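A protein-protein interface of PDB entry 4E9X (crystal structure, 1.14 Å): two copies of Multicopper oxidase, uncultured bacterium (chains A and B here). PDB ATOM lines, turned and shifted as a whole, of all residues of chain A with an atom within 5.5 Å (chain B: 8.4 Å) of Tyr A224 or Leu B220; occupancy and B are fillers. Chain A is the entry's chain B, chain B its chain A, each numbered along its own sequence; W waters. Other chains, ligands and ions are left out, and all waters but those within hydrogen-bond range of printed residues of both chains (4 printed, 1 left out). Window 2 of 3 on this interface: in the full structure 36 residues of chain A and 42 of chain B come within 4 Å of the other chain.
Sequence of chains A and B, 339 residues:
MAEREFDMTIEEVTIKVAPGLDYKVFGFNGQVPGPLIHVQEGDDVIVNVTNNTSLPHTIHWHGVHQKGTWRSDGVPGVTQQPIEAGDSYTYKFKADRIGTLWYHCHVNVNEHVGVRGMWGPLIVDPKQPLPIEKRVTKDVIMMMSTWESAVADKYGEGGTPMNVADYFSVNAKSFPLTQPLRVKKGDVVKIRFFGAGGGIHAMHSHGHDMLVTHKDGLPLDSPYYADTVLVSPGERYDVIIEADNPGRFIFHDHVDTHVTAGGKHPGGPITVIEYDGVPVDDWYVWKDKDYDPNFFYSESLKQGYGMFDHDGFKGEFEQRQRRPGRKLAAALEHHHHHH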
ATOM      1  N   MET A 210     -27.336  31.416  28.732  1.00  0.00           N
ATOM      2  CA  MET A 210     -28.095  31.834  27.553  1.00  0.00           C
ATOM      3  C   MET A 210     -27.906  30.786  26.450  1.00  0.00           C
ATOM      4  O   MET A 210     -26.752  30.339  26.263  1.00  0.00           O
ATOM      5  CB  MET A 210     -27.576  33.164  27.040  1.00  0.00           C
ATOM      6  CG  MET A 210     -27.921  34.312  28.009  1.00  0.00           C
ATOM      7  SD  MET A 210     -27.115  35.867  27.539  1.00  0.00           S
ATOM      8  CE  MET A 210     -25.460  35.621  28.223  1.00  0.00           C
ATOM      9  N   LEU A 211     -28.937  30.434  25.745  1.00  0.00           N
ATOM     10  CA  LEU A 211     -28.781  29.597  24.535  1.00  0.00           C
ATOM     11  C   LEU A 211     -28.745  30.568  23.357  1.00  0.00           C
ATOM     12  O   LEU A 211     -29.745  31.266  23.090  1.00  0.00           O
ATOM     13  CB  LEU A 211     -29.954  28.615  24.399  1.00  0.00           C
ATOM     14  CG  LEU A 211     -29.850  27.734  23.168  1.00  0.00           C
ATOM     15  CD1 LEU A 211     -28.620  26.811  23.233  1.00  0.00           C
ATOM     16  CD2 LEU A 211     -31.120  26.930  22.964  1.00  0.00           C
ATOM     17  N   VAL A 212     -27.594  30.651  22.664  1.00  0.00           N
ATOM     18  CA  VAL A 212     -27.456  31.523  21.491  1.00  0.00           C
ATOM     19  C   VAL A 212     -28.071  30.793  20.301  1.00  0.00           C
ATOM     20  O   VAL A 212     -27.576  29.746  19.876  1.00  0.00           O
ATOM     21  CB  VAL A 212     -25.967  31.857  21.241  1.00  0.00           C
ATOM     22  CG1 VAL A 212     -25.882  32.799  20.072  1.00  0.00           C
ATOM     23  CG2 VAL A 212     -25.312  32.450  22.489  1.00  0.00           C
ATOM     24  N   THR A 213     -29.158  31.408  19.794  1.00  0.00           N
ATOM     25  CA  THR A 213     -29.940  30.769  18.749  1.00  0.00           C
ATOM     26  C   THR A 213     -29.813  31.426  17.384  1.00  0.00           C
ATOM     27  O   THR A 213     -30.067  30.770  16.377  1.00  0.00           O
ATOM     28  CB  THR A 213     -31.442  30.719  19.128  1.00  0.00           C
ATOM     29  OG1 THR A 213     -31.908  32.062  19.343  1.00  0.00           O
ATOM     30  CG2 THR A 213     -31.657  29.921  20.426  1.00  0.00           C
ATOM     31  N   LEU A 220     -29.022  29.732  13.882  1.00  0.00           N
ATOM     32  CA  LEU A 220     -27.834  28.884  13.779  1.00  0.00           C
ATOM     33  C   LEU A 220     -28.222  27.433  13.675  1.00  0.00           C
ATOM     34  O   LEU A 220     -29.087  26.912  14.401  1.00  0.00           O
ATOM     35  CB  LEU A 220     -27.031  29.033  15.090  1.00  0.00           C
ATOM     36  CG  LEU A 220     -26.393  30.429  15.242  1.00  0.00           C
ATOM     37  CD1 LEU A 220     -25.733  30.537  16.634  1.00  0.00           C
ATOM     38  CD2 LEU A 220     -25.388  30.701  14.151  1.00  0.00           C
ATOM     39  N   SER A 222     -26.182  25.181  14.617  1.00  0.00           N
ATOM     40  CA  SER A 222     -25.572  24.687  15.849  1.00  0.00           C
ATOM     41  C   SER A 222     -25.647  25.735  16.944  1.00  0.00           C
ATOM     42  O   SER A 222     -24.655  26.421  17.230  1.00  0.00           O
ATOM     43  CB  SER A 222     -24.090  24.302  15.652  1.00  0.00           C
ATOM     44  OG  SER A 222     -23.646  23.503  16.735  1.00  0.00           O
ATOM     45  N   PRO A 223     -26.771  25.891  17.597  1.00  0.00           N
ATOM     46  CA  PRO A 223     -26.859  26.846  18.725  1.00  0.00           C
ATOM     47  C   PRO A 223     -25.952  26.363  19.811  1.00  0.00           C
ATOM     48  O   PRO A 223     -25.577  25.189  19.915  1.00  0.00           O
ATOM     49  CB  PRO A 223     -28.310  26.759  19.143  1.00  0.00           C
ATOM     50  CG  PRO A 223     -28.723  25.394  18.715  1.00  0.00           C
ATOM     51  CD  PRO A 223     -28.059  25.183  17.363  1.00  0.00           C
ATOM     52  N   TYR A 224     -25.565  27.308  20.665  1.00  0.00           N
ATOM     53  CA  TYR A 224     -24.621  26.989  21.734  1.00  0.00           C
ATOM     54  C   TYR A 224     -24.941  27.833  22.987  1.00  0.00           C
ATOM     55  O   TYR A 224     -25.458  28.952  22.915  1.00  0.00           O
ATOM     56  CB  TYR A 224     -23.172  27.241  21.309  1.00  0.00           C
ATOM     57  CG  TYR A 224     -22.900  28.671  20.905  1.00  0.00           C
ATOM     58  CD1 TYR A 224     -22.376  29.585  21.809  1.00  0.00           C
ATOM     59  CD2 TYR A 224     -23.187  29.112  19.608  1.00  0.00           C
ATOM     60  CE1 TYR A 224     -22.125  30.915  21.438  1.00  0.00           C
ATOM     61  CE2 TYR A 224     -22.953  30.426  19.211  1.00  0.00           C
ATOM     62  CZ  TYR A 224     -22.419  31.322  20.156  1.00  0.00           C
ATOM     63  OH  TYR A 224     -22.185  32.637  19.751  1.00  0.00           O
ATOM     64  N   TYR A 225     -24.592  27.270  24.131  1.00  0.00           N
ATOM     65  CA  TYR A 225     -24.766  27.978  25.400  1.00  0.00           C
ATOM     66  C   TYR A 225     -23.598  28.889  25.687  1.00  0.00           C
ATOM     67  O   TYR A 225     -22.442  28.610  25.344  1.00  0.00           O
ATOM     68  CB  TYR A 225     -24.899  26.969  26.553  1.00  0.00           C
ATOM     69  CG  TYR A 225     -26.198  26.217  26.577  1.00  0.00           C
ATOM     70  CD1 TYR A 225     -27.359  26.872  27.030  1.00  0.00           C
ATOM     71  CD2 TYR A 225     -26.298  24.908  26.174  1.00  0.00           C
ATOM     72  CE1 TYR A 225     -28.573  26.189  27.066  1.00  0.00           C
ATOM     73  CE2 TYR A 225     -27.499  24.225  26.205  1.00  0.00           C
ATOM     74  CZ  TYR A 225     -28.648  24.884  26.648  1.00  0.00           C
ATOM     75  OH  TYR A 225     -29.871  24.232  26.701  1.00  0.00           O
ATOM     76  N   ALA A 226     -23.915  29.968  26.381  1.00  0.00           N
ATOM     77  CA  ALA A 226     -22.929  30.964  26.771  1.00  0.00           C
ATOM     78  C   ALA A 226     -23.406  31.637  28.026  1.00  0.00           C
ATOM     79  O   ALA A 226     -24.626  31.814  28.217  1.00  0.00           O
ATOM     80  CB  ALA A 226     -22.769  32.049  25.678  1.00  0.00           C
ATOM     81  N   TYR A 237     -27.301  39.344  18.219  1.00  0.00           N
ATOM     82  CA  TYR A 237     -27.371  37.978  18.714  1.00  0.00           C
ATOM     83  C   TYR A 237     -28.728  37.776  19.377  1.00  0.00           C
ATOM     84  O   TYR A 237     -29.112  38.677  20.159  1.00  0.00           O
ATOM     85  CB  TYR A 237     -26.251  37.654  19.748  1.00  0.00           C
ATOM     86  CG  TYR A 237     -24.909  37.525  19.016  1.00  0.00           C
ATOM     87  CD1 TYR A 237     -24.477  36.296  18.533  1.00  0.00           C
ATOM     88  CD2 TYR A 237     -24.117  38.647  18.798  1.00  0.00           C
ATOM     89  CE1 TYR A 237     -23.252  36.176  17.842  1.00  0.00           C
ATOM     90  CE2 TYR A 237     -22.885  38.574  18.100  1.00  0.00           C
ATOM     91  CZ  TYR A 237     -22.495  37.330  17.663  1.00  0.00           C
ATOM     92  OH  TYR A 237     -21.290  37.221  16.950  1.00  0.00           O
ATOM     93  N   LEU B 130     -16.093  15.028  27.937  1.00  0.00           N
ATOM     94  CA  LEU B 130     -16.010  14.636  26.533  1.00  0.00           C
ATOM     95  C   LEU B 130     -15.028  13.501  26.413  1.00  0.00           C
ATOM     96  O   LEU B 130     -14.063  13.523  27.157  1.00  0.00           O
ATOM     97  CB  LEU B 130     -15.524  15.763  25.621  1.00  0.00           C
ATOM     98  CG  LEU B 130     -16.437  17.008  25.623  1.00  0.00           C
ATOM     99  CD1 LEU B 130     -15.983  18.062  24.645  1.00  0.00           C
ATOM    100  CD2 LEU B 130     -17.852  16.576  25.251  1.00  0.00           C
ATOM    101  N   LEU B 211      -8.185  23.037  18.772  1.00  0.00           N
ATOM    102  CA  LEU B 211      -9.565  22.599  18.623  1.00  0.00           C
ATOM    103  C   LEU B 211     -10.369  23.245  19.748  1.00  0.00           C
ATOM    104  O   LEU B 211     -10.147  22.905  20.916  1.00  0.00           O
ATOM    105  CB  LEU B 211      -9.673  21.075  18.714  1.00  0.00           C
ATOM    106  CG  LEU B 211     -11.115  20.564  18.552  1.00  0.00           C
ATOM    107  CD1 LEU B 211     -11.675  20.889  17.158  1.00  0.00           C
ATOM    108  CD2 LEU B 211     -11.181  19.062  18.813  1.00  0.00           C
ATOM    109  N   VAL B 212     -11.240  24.180  19.398  1.00  0.00           N
ATOM    110  CA  VAL B 212     -12.090  24.872  20.391  1.00  0.00           C
ATOM    111  C   VAL B 212     -13.239  23.929  20.752  1.00  0.00           C
ATOM    112  O   VAL B 212     -14.088  23.603  19.912  1.00  0.00           O
ATOM    113  CB  VAL B 212     -12.601  26.196  19.819  1.00  0.00           C
ATOM    114  CG1 VAL B 212     -13.432  26.874  20.915  1.00  0.00           C
ATOM    115  CG2 VAL B 212     -11.465  27.101  19.321  1.00  0.00           C
ATOM    116  N   THR B 213     -13.248  23.469  22.017  1.00  0.00           N
ATOM    117  CA  THR B 213     -14.238  22.489  22.437  1.00  0.00           C
ATOM    118  C   THR B 213     -15.293  23.025  23.383  1.00  0.00           C
ATOM    119  O   THR B 213     -16.333  22.402  23.499  1.00  0.00           O
ATOM    120  CB  THR B 213     -13.501  21.323  23.172  1.00  0.00           C
ATOM    121  OG1 THR B 213     -12.762  21.831  24.279  1.00  0.00           O
ATOM    122  CG2 THR B 213     -12.479  20.632  22.255  1.00  0.00           C
ATOM    123  N   HIS B 214     -15.007  24.115  24.111  1.00  0.00           N
ATOM    124  CA  HIS B 214     -15.956  24.614  25.117  1.00  0.00           C
ATOM    125  C   HIS B 214     -16.011  26.138  25.103  1.00  0.00           C
ATOM    126  O   HIS B 214     -14.958  26.778  24.979  1.00  0.00           O
ATOM    127  CB  HIS B 214     -15.583  24.229  26.557  1.00  0.00           C
ATOM    128  CG  HIS B 214     -15.524  22.758  26.872  1.00  0.00           C
ATOM    129  ND1 HIS B 214     -14.562  21.915  26.311  1.00  0.00           N
ATOM    130  CD2 HIS B 214     -16.304  22.007  27.700  1.00  0.00           C
ATOM    131  CE1 HIS B 214     -14.782  20.719  26.810  1.00  0.00           C
ATOM    132  NE2 HIS B 214     -15.831  20.734  27.648  1.00  0.00           N
ATOM    133  N   LYS B 215     -17.213  26.625  25.251  1.00  0.00           N
ATOM    134  CA  LYS B 215     -17.467  28.061  25.369  1.00  0.00           C
ATOM    135  C   LYS B 215     -18.070  28.289  26.757  1.00  0.00           C
ATOM    136  O   LYS B 215     -19.083  27.662  27.094  1.00  0.00           O
ATOM    137  CB  LYS B 215     -18.421  28.522  24.256  1.00  0.00           C
ATOM    138  CG  LYS B 215     -19.141  29.821  24.499  1.00  0.00           C
ATOM    139  CD  LYS B 215     -18.235  31.052  24.658  1.00  0.00           C
ATOM    140  CE  LYS B 215     -19.150  32.266  24.825  1.00  0.00           C
ATOM    141  NZ  LYS B 215     -18.451  33.335  25.565  1.00  0.00           N
ATOM    142  N   ASP B 216     -17.398  29.147  27.550  1.00  0.00           N
ATOM    143  CA  ASP B 216     -17.856  29.451  28.922  1.00  0.00           C
ATOM    144  C   ASP B 216     -18.053  28.161  29.728  1.00  0.00           C
ATOM    145  O   ASP B 216     -18.930  28.067  30.595  1.00  0.00           O
ATOM    146  CB  ASP B 216     -19.129  30.288  28.909  1.00  0.00           C
ATOM    147  CG  ASP B 216     -18.891  31.670  28.229  1.00  0.00           C
ATOM    148  OD1 ASP B 216     -17.724  32.061  28.023  1.00  0.00           O
ATOM    149  OD2 ASP B 216     -19.939  32.265  27.910  1.00  0.00           O
ATOM    150  N   GLY B 217     -17.187  27.163  29.475  1.00  0.00           N
ATOM    151  CA  GLY B 217     -17.196  25.908  30.226  1.00  0.00           C
ATOM    152  C   GLY B 217     -18.144  24.854  29.701  1.00  0.00           C
ATOM    153  O   GLY B 217     -18.046  23.724  30.163  1.00  0.00           O
ATOM    154  N   LEU B 218     -19.007  25.164  28.734  1.00  0.00           N
ATOM    155  CA  LEU B 218     -19.968  24.141  28.254  1.00  0.00           C
ATOM    156  C   LEU B 218     -19.528  23.651  26.889  1.00  0.00           C
ATOM    157  O   LEU B 218     -19.063  24.419  26.037  1.00  0.00           O
ATOM    158  CB  LEU B 218     -21.376  24.737  28.172  1.00  0.00           C
ATOM    159  CG  LEU B 218     -22.005  24.997  29.536  1.00  0.00           C
ATOM    160  CD1 LEU B 218     -23.355  25.703  29.410  1.00  0.00           C
ATOM    161  CD2 LEU B 218     -22.193  23.683  30.314  1.00  0.00           C
ATOM    162  N   PRO B 219     -19.643  22.340  26.666  1.00  0.00           N
ATOM    163  CA  PRO B 219     -19.083  21.754  25.453  1.00  0.00           C
ATOM    164  C   PRO B 219     -19.888  22.113  24.215  1.00  0.00           C
ATOM    165  O   PRO B 219     -21.134  22.016  24.200  1.00  0.00           O
ATOM    166  CB  PRO B 219     -19.170  20.239  25.709  1.00  0.00           C
ATOM    167  CG  PRO B 219     -20.299  20.105  26.719  1.00  0.00           C
ATOM    168  CD  PRO B 219     -20.208  21.317  27.594  1.00  0.00           C
ATOM    169  N   LEU B 220     -19.188  22.487  23.157  1.00  0.00           N
ATOM    170  CA  LEU B 220     -19.846  22.844  21.907  1.00  0.00           C
ATOM    171  C   LEU B 220     -20.302  21.579  21.198  1.00  0.00           C
ATOM    172  O   LEU B 220     -19.564  20.583  21.076  1.00  0.00           O
ATOM    173  CB  LEU B 220     -18.859  23.570  21.003  1.00  0.00           C
ATOM    174  CG  LEU B 220     -18.413  24.975  21.493  1.00  0.00           C
ATOM    175  CD1 LEU B 220     -17.300  25.460  20.594  1.00  0.00           C
ATOM    176  CD2 LEU B 220     -19.558  25.950  21.472  1.00  0.00           C
ATOM    177  N   ASP B 221     -21.500  21.629  20.626  1.00  0.00           N
ATOM    178  CA  ASP B 221     -21.943  20.544  19.739  1.00  0.00           C
ATOM    179  C   ASP B 221     -21.109  20.524  18.462  1.00  0.00           C
ATOM    180  O   ASP B 221     -20.946  19.421  17.874  1.00  0.00           O
ATOM    181  CB  ASP B 221     -23.427  20.716  19.410  1.00  0.00           C
ATOM    182  CG  ASP B 221     -24.385  20.396  20.538  1.00  0.00           C
ATOM    183  OD1 ASP B 221     -24.045  19.645  21.495  1.00  0.00           O
ATOM    184  OD2 ASP B 221     -25.551  20.899  20.469  1.00  0.00           O
ATOM    185  N   SER B 222     -20.622  21.674  18.031  1.00  0.00           N
ATOM    186  CA  SER B 222     -19.820  21.751  16.812  1.00  0.00           C
ATOM    187  C   SER B 222     -18.483  22.412  17.121  1.00  0.00           C
ATOM    188  O   SER B 222     -18.261  23.597  16.899  1.00  0.00           O
ATOM    189  CB  SER B 222     -20.541  22.544  15.732  1.00  0.00           C
ATOM    190  OG  SER B 222     -19.845  22.387  14.510  1.00  0.00           O
ATOM    191  N   PRO B 223     -17.536  21.638  17.668  1.00  0.00           N
ATOM    192  CA  PRO B 223     -16.192  22.169  17.913  1.00  0.00           C
ATOM    193  C   PRO B 223     -15.563  22.585  16.600  1.00  0.00           C
ATOM    194  O   PRO B 223     -15.913  22.095  15.514  1.00  0.00           O
ATOM    195  CB  PRO B 223     -15.456  20.999  18.554  1.00  0.00           C
ATOM    196  CG  PRO B 223     -16.228  19.779  18.195  1.00  0.00           C
ATOM    197  CD  PRO B 223     -17.672  20.213  18.080  1.00  0.00           C
ATOM    198  N   TYR B 224     -14.600  23.505  16.653  1.00  0.00           N
ATOM    199  CA  TYR B 224     -13.977  23.978  15.439  1.00  0.00           C
ATOM    200  C   TYR B 224     -12.532  24.295  15.703  1.00  0.00           C
ATOM    201  O   TYR B 224     -12.129  24.680  16.807  1.00  0.00           O
ATOM    202  CB  TYR B 224     -14.722  25.242  14.902  1.00  0.00           C
ATOM    203  CG  TYR B 224     -14.693  26.411  15.889  1.00  0.00           C
ATOM    204  CD1 TYR B 224     -13.720  27.400  15.807  1.00  0.00           C
ATOM    205  CD2 TYR B 224     -15.659  26.482  16.899  1.00  0.00           C
ATOM    206  CE1 TYR B 224     -13.703  28.460  16.714  1.00  0.00           C
ATOM    207  CE2 TYR B 224     -15.673  27.525  17.814  1.00  0.00           C
ATOM    208  CZ  TYR B 224     -14.675  28.496  17.700  1.00  0.00           C
ATOM    209  OH  TYR B 224     -14.698  29.526  18.618  1.00  0.00           O
ATOM    210  N   TYR B 225     -11.722  24.172  14.648  1.00  0.00           N
ATOM    211  CA  TYR B 225     -10.313  24.534  14.732  1.00  0.00           C
ATOM    212  C   TYR B 225     -10.080  26.018  14.541  1.00  0.00           C
ATOM    213  O   TYR B 225     -10.794  26.707  13.791  1.00  0.00           O
ATOM    214  CB  TYR B 225      -9.543  23.771  13.652  1.00  0.00           C
ATOM    215  CG  TYR B 225      -9.369  22.293  13.946  1.00  0.00           C
ATOM    216  CD1 TYR B 225      -8.448  21.878  14.927  1.00  0.00           C
ATOM    217  CD2 TYR B 225     -10.125  21.381  13.229  1.00  0.00           C
ATOM    218  CE1 TYR B 225      -8.273  20.531  15.200  1.00  0.00           C
ATOM    219  CE2 TYR B 225      -9.942  20.026  13.502  1.00  0.00           C
ATOM    220  CZ  TYR B 225      -9.037  19.604  14.473  1.00  0.00           C
ATOM    221  OH  TYR B 225      -8.924  18.225  14.688  1.00  0.00           O
ATOM    222  N   GLU B 235     -15.425  35.997  29.265  1.00  0.00           N
ATOM    223  CA  GLU B 235     -15.532  34.741  28.533  1.00  0.00           C
ATOM    224  C   GLU B 235     -14.498  33.706  28.945  1.00  0.00           C
ATOM    225  O   GLU B 235     -13.428  34.064  29.413  1.00  0.00           O
ATOM    226  CB  GLU B 235     -15.312  34.968  27.036  1.00  0.00           C
ATOM    227  CG  GLU B 235     -16.310  35.959  26.400  1.00  0.00           C
ATOM    228  CD  GLU B 235     -16.116  35.840  24.890  1.00  0.00           C
ATOM    229  OE1 GLU B 235     -15.181  36.482  24.422  1.00  0.00           O
ATOM    230  OE2 GLU B 235     -16.802  35.066  24.218  1.00  0.00           O
ATOM    231  N   ARG B 236     -14.822  32.435  28.707  1.00  0.00           N
ATOM    232  CA  ARG B 236     -13.779  31.404  28.709  1.00  0.00           C
ATOM    233  C   ARG B 236     -13.920  30.594  27.433  1.00  0.00           C
ATOM    234  O   ARG B 236     -15.009  30.376  26.894  1.00  0.00           O
ATOM    235  CB  ARG B 236     -13.877  30.468  29.935  1.00  0.00           C
ATOM    236  CG  ARG B 236     -13.446  31.146  31.237  1.00  0.00           C
ATOM    237  CD  ARG B 236     -14.550  31.951  31.912  1.00  0.00           C
ATOM    238  NE  ARG B 236     -15.661  31.092  32.285  1.00  0.00           N
ATOM    239  CZ  ARG B 236     -16.968  31.375  32.122  1.00  0.00           C
ATOM    240  NH1 ARG B 236     -17.401  32.521  31.620  1.00  0.00           N
ATOM    241  NH2 ARG B 236     -17.871  30.446  32.491  1.00  0.00           N
ATOM    242  N   TYR B 237     -12.758  30.140  26.942  1.00  0.00           N
ATOM    243  CA  TYR B 237     -12.712  29.158  25.870  1.00  0.00           C
ATOM    244  C   TYR B 237     -11.795  28.019  26.301  1.00  0.00           C
ATOM    245  O   TYR B 237     -10.706  28.312  26.821  1.00  0.00           O
ATOM    246  CB  TYR B 237     -12.161  29.761  24.557  1.00  0.00           C
ATOM    247  CG  TYR B 237     -13.194  30.704  23.971  1.00  0.00           C
ATOM    248  CD1 TYR B 237     -14.156  30.211  23.064  1.00  0.00           C
ATOM    249  CD2 TYR B 237     -13.231  32.069  24.309  1.00  0.00           C
ATOM    250  CE1 TYR B 237     -15.128  31.066  22.508  1.00  0.00           C
ATOM    251  CE2 TYR B 237     -14.184  32.910  23.765  1.00  0.00           C
ATOM    252  CZ  TYR B 237     -15.129  32.398  22.877  1.00  0.00           C
ATOM    253  OH  TYR B 237     -16.098  33.247  22.333  1.00  0.00           O
ATOM    254  N   ASP B 238     -12.193  26.759  26.070  1.00  0.00           N
ATOM    255  CA  ASP B 238     -11.284  25.651  26.257  1.00  0.00           C
ATOM    256  C   ASP B 238     -10.924  25.122  24.895  1.00  0.00           C
ATOM    257  O   ASP B 238     -11.792  24.972  24.031  1.00  0.00           O
ATOM    258  CB  ASP B 238     -11.893  24.489  27.040  1.00  0.00           C
ATOM    259  CG  ASP B 238     -12.405  24.712  28.450  1.00  0.00           C
ATOM    260  OD1 ASP B 238     -12.514  25.864  28.915  1.00  0.00           O
ATOM    261  OD2 ASP B 238     -12.661  23.686  29.102  1.00  0.00           O
HETATM  262  O   HOH W   1     -23.174  24.730  23.808  1.00  0.00           O
HETATM  263  O   HOH W   2     -23.239  23.927  21.129  1.00  0.00           O
HETATM  264  O   HOH W   3     -21.784  24.304  18.700  1.00  0.00           O
HETATM  265  O   HOH W   4     -26.346  22.719  18.774  1.00  0.00           O
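The side-chain carboxylate of Asp B216 is in salt-bridge range of the guanidinium group of Arg B236 (3.6 Å). N of Met A210 sits at hydrogen-bond distance from O of Ala A226 (2.8 Å). The side-chain carboxylate (OE2) of Glu B235 lies within salt-bridge range of the side-chain amino group (NZ) of Lys B215 (2.7 Å). The side-chain carboxylate (OD1) of Asp B216 is in salt-bridge range of the side-chain amino group (NZ) of Lys B215 (2.9 Å). The backbone NH of Leu B220 lies within hydrogen-bond range of the backbone carbonyl oxygen of Thr B213, at 2.9 Å. N of Val A212 lies within hydrogen-bond range of O of Tyr A224, at 2.7 Å.
Among the printed residues, merely in contact across the chains: Ser A222 with Asp B221, Ser A222 with Ser B222, Tyr A224 with Leu B220, Tyr A225 with Lys B215, Tyr A225 with Leu B218, Ala A226 with Lys B215 and Ala A226 with Asp B216.
Of chain B, only Leu B220 (3.8 Å) comes within 4 Å of Tyr A224. Of the printed residues of chain A, Leu B220 touches Tyr A224 (3.8 Å). No residue of chain B comes within 4 Å of Val A212. Printed residues of chain B within 4 Å of Ser A222: Asp B221 (3.9 Å) and Ser B222 (3.4 Å). Of the printed residues of chain B, Tyr A225 touches Lys B215 (3.6 Å) and Leu B218 (3.5 Å). Printed residues of chain A within 4 Å of Lys B215: Tyr A225 (3.6 Å) and Ala A226 (3.7 Å). Of the printed residues of chain A, Asp B216 touches Ala A226 (3.5 Å). Leu B211 touches none of the printed residues of chain A. Leu A220 touches none of the printed residues of chain B. The nearest residue of chain B that does not touch Tyr A224 is Lys B215 (4.2 Å). The nearest printed residue of chain B that does not touch Ala A226 is Leu B218 (5.3 Å).
Printed residues of chain A that touch a printed residue of chain B: Ser A222, Tyr A224, Tyr A225 and Ala A226. Hydrophobic or aromatic side chains of chain A within 4 Å of the printed part of chain B: Tyr A224, Tyr A225 and Ala A226. Among the printed residues, 7 pairs touch across the chains.
Ser B222 touches its own counterpart, Ser A222. Tyr A224 touches Leu B220, but with the chains exchanged Leu A220 does not touch Tyr B224 (10.6 Å). Positions printed for both chains: 211, 212, 213, 220, 222, 223, 224, 225 and 237. Of the 7 pairs that touch across the chains among the printed residues, 1 has its exchanged pair printed and touching as well.
Water W4 lies within hydrogen-bond range of the side-chain carboxylate of Asp B221 (2.6 Å), the backbone carbonyl oxygen of Pro A223 (2.8 Å) and the side-chain hydroxyl of Ser A222 (3.5 Å). Water W3 lies within hydrogen-bond range of the side-chain hydroxyl of Ser A222 (2.8 Å), the backbone NH of Ser B222 (3.0 Å) and the backbone NH of Asp B221 (3.3 Å). Water W2 bridges O of Pro A223 (2.9 Å) and N of Asp B221 (2.9 Å). Water W1 bridges the backbone NH (N) of Tyr A225 (2.9 Å) and the backbone carbonyl oxygen (O) of Pro B219 (3.4 Å).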
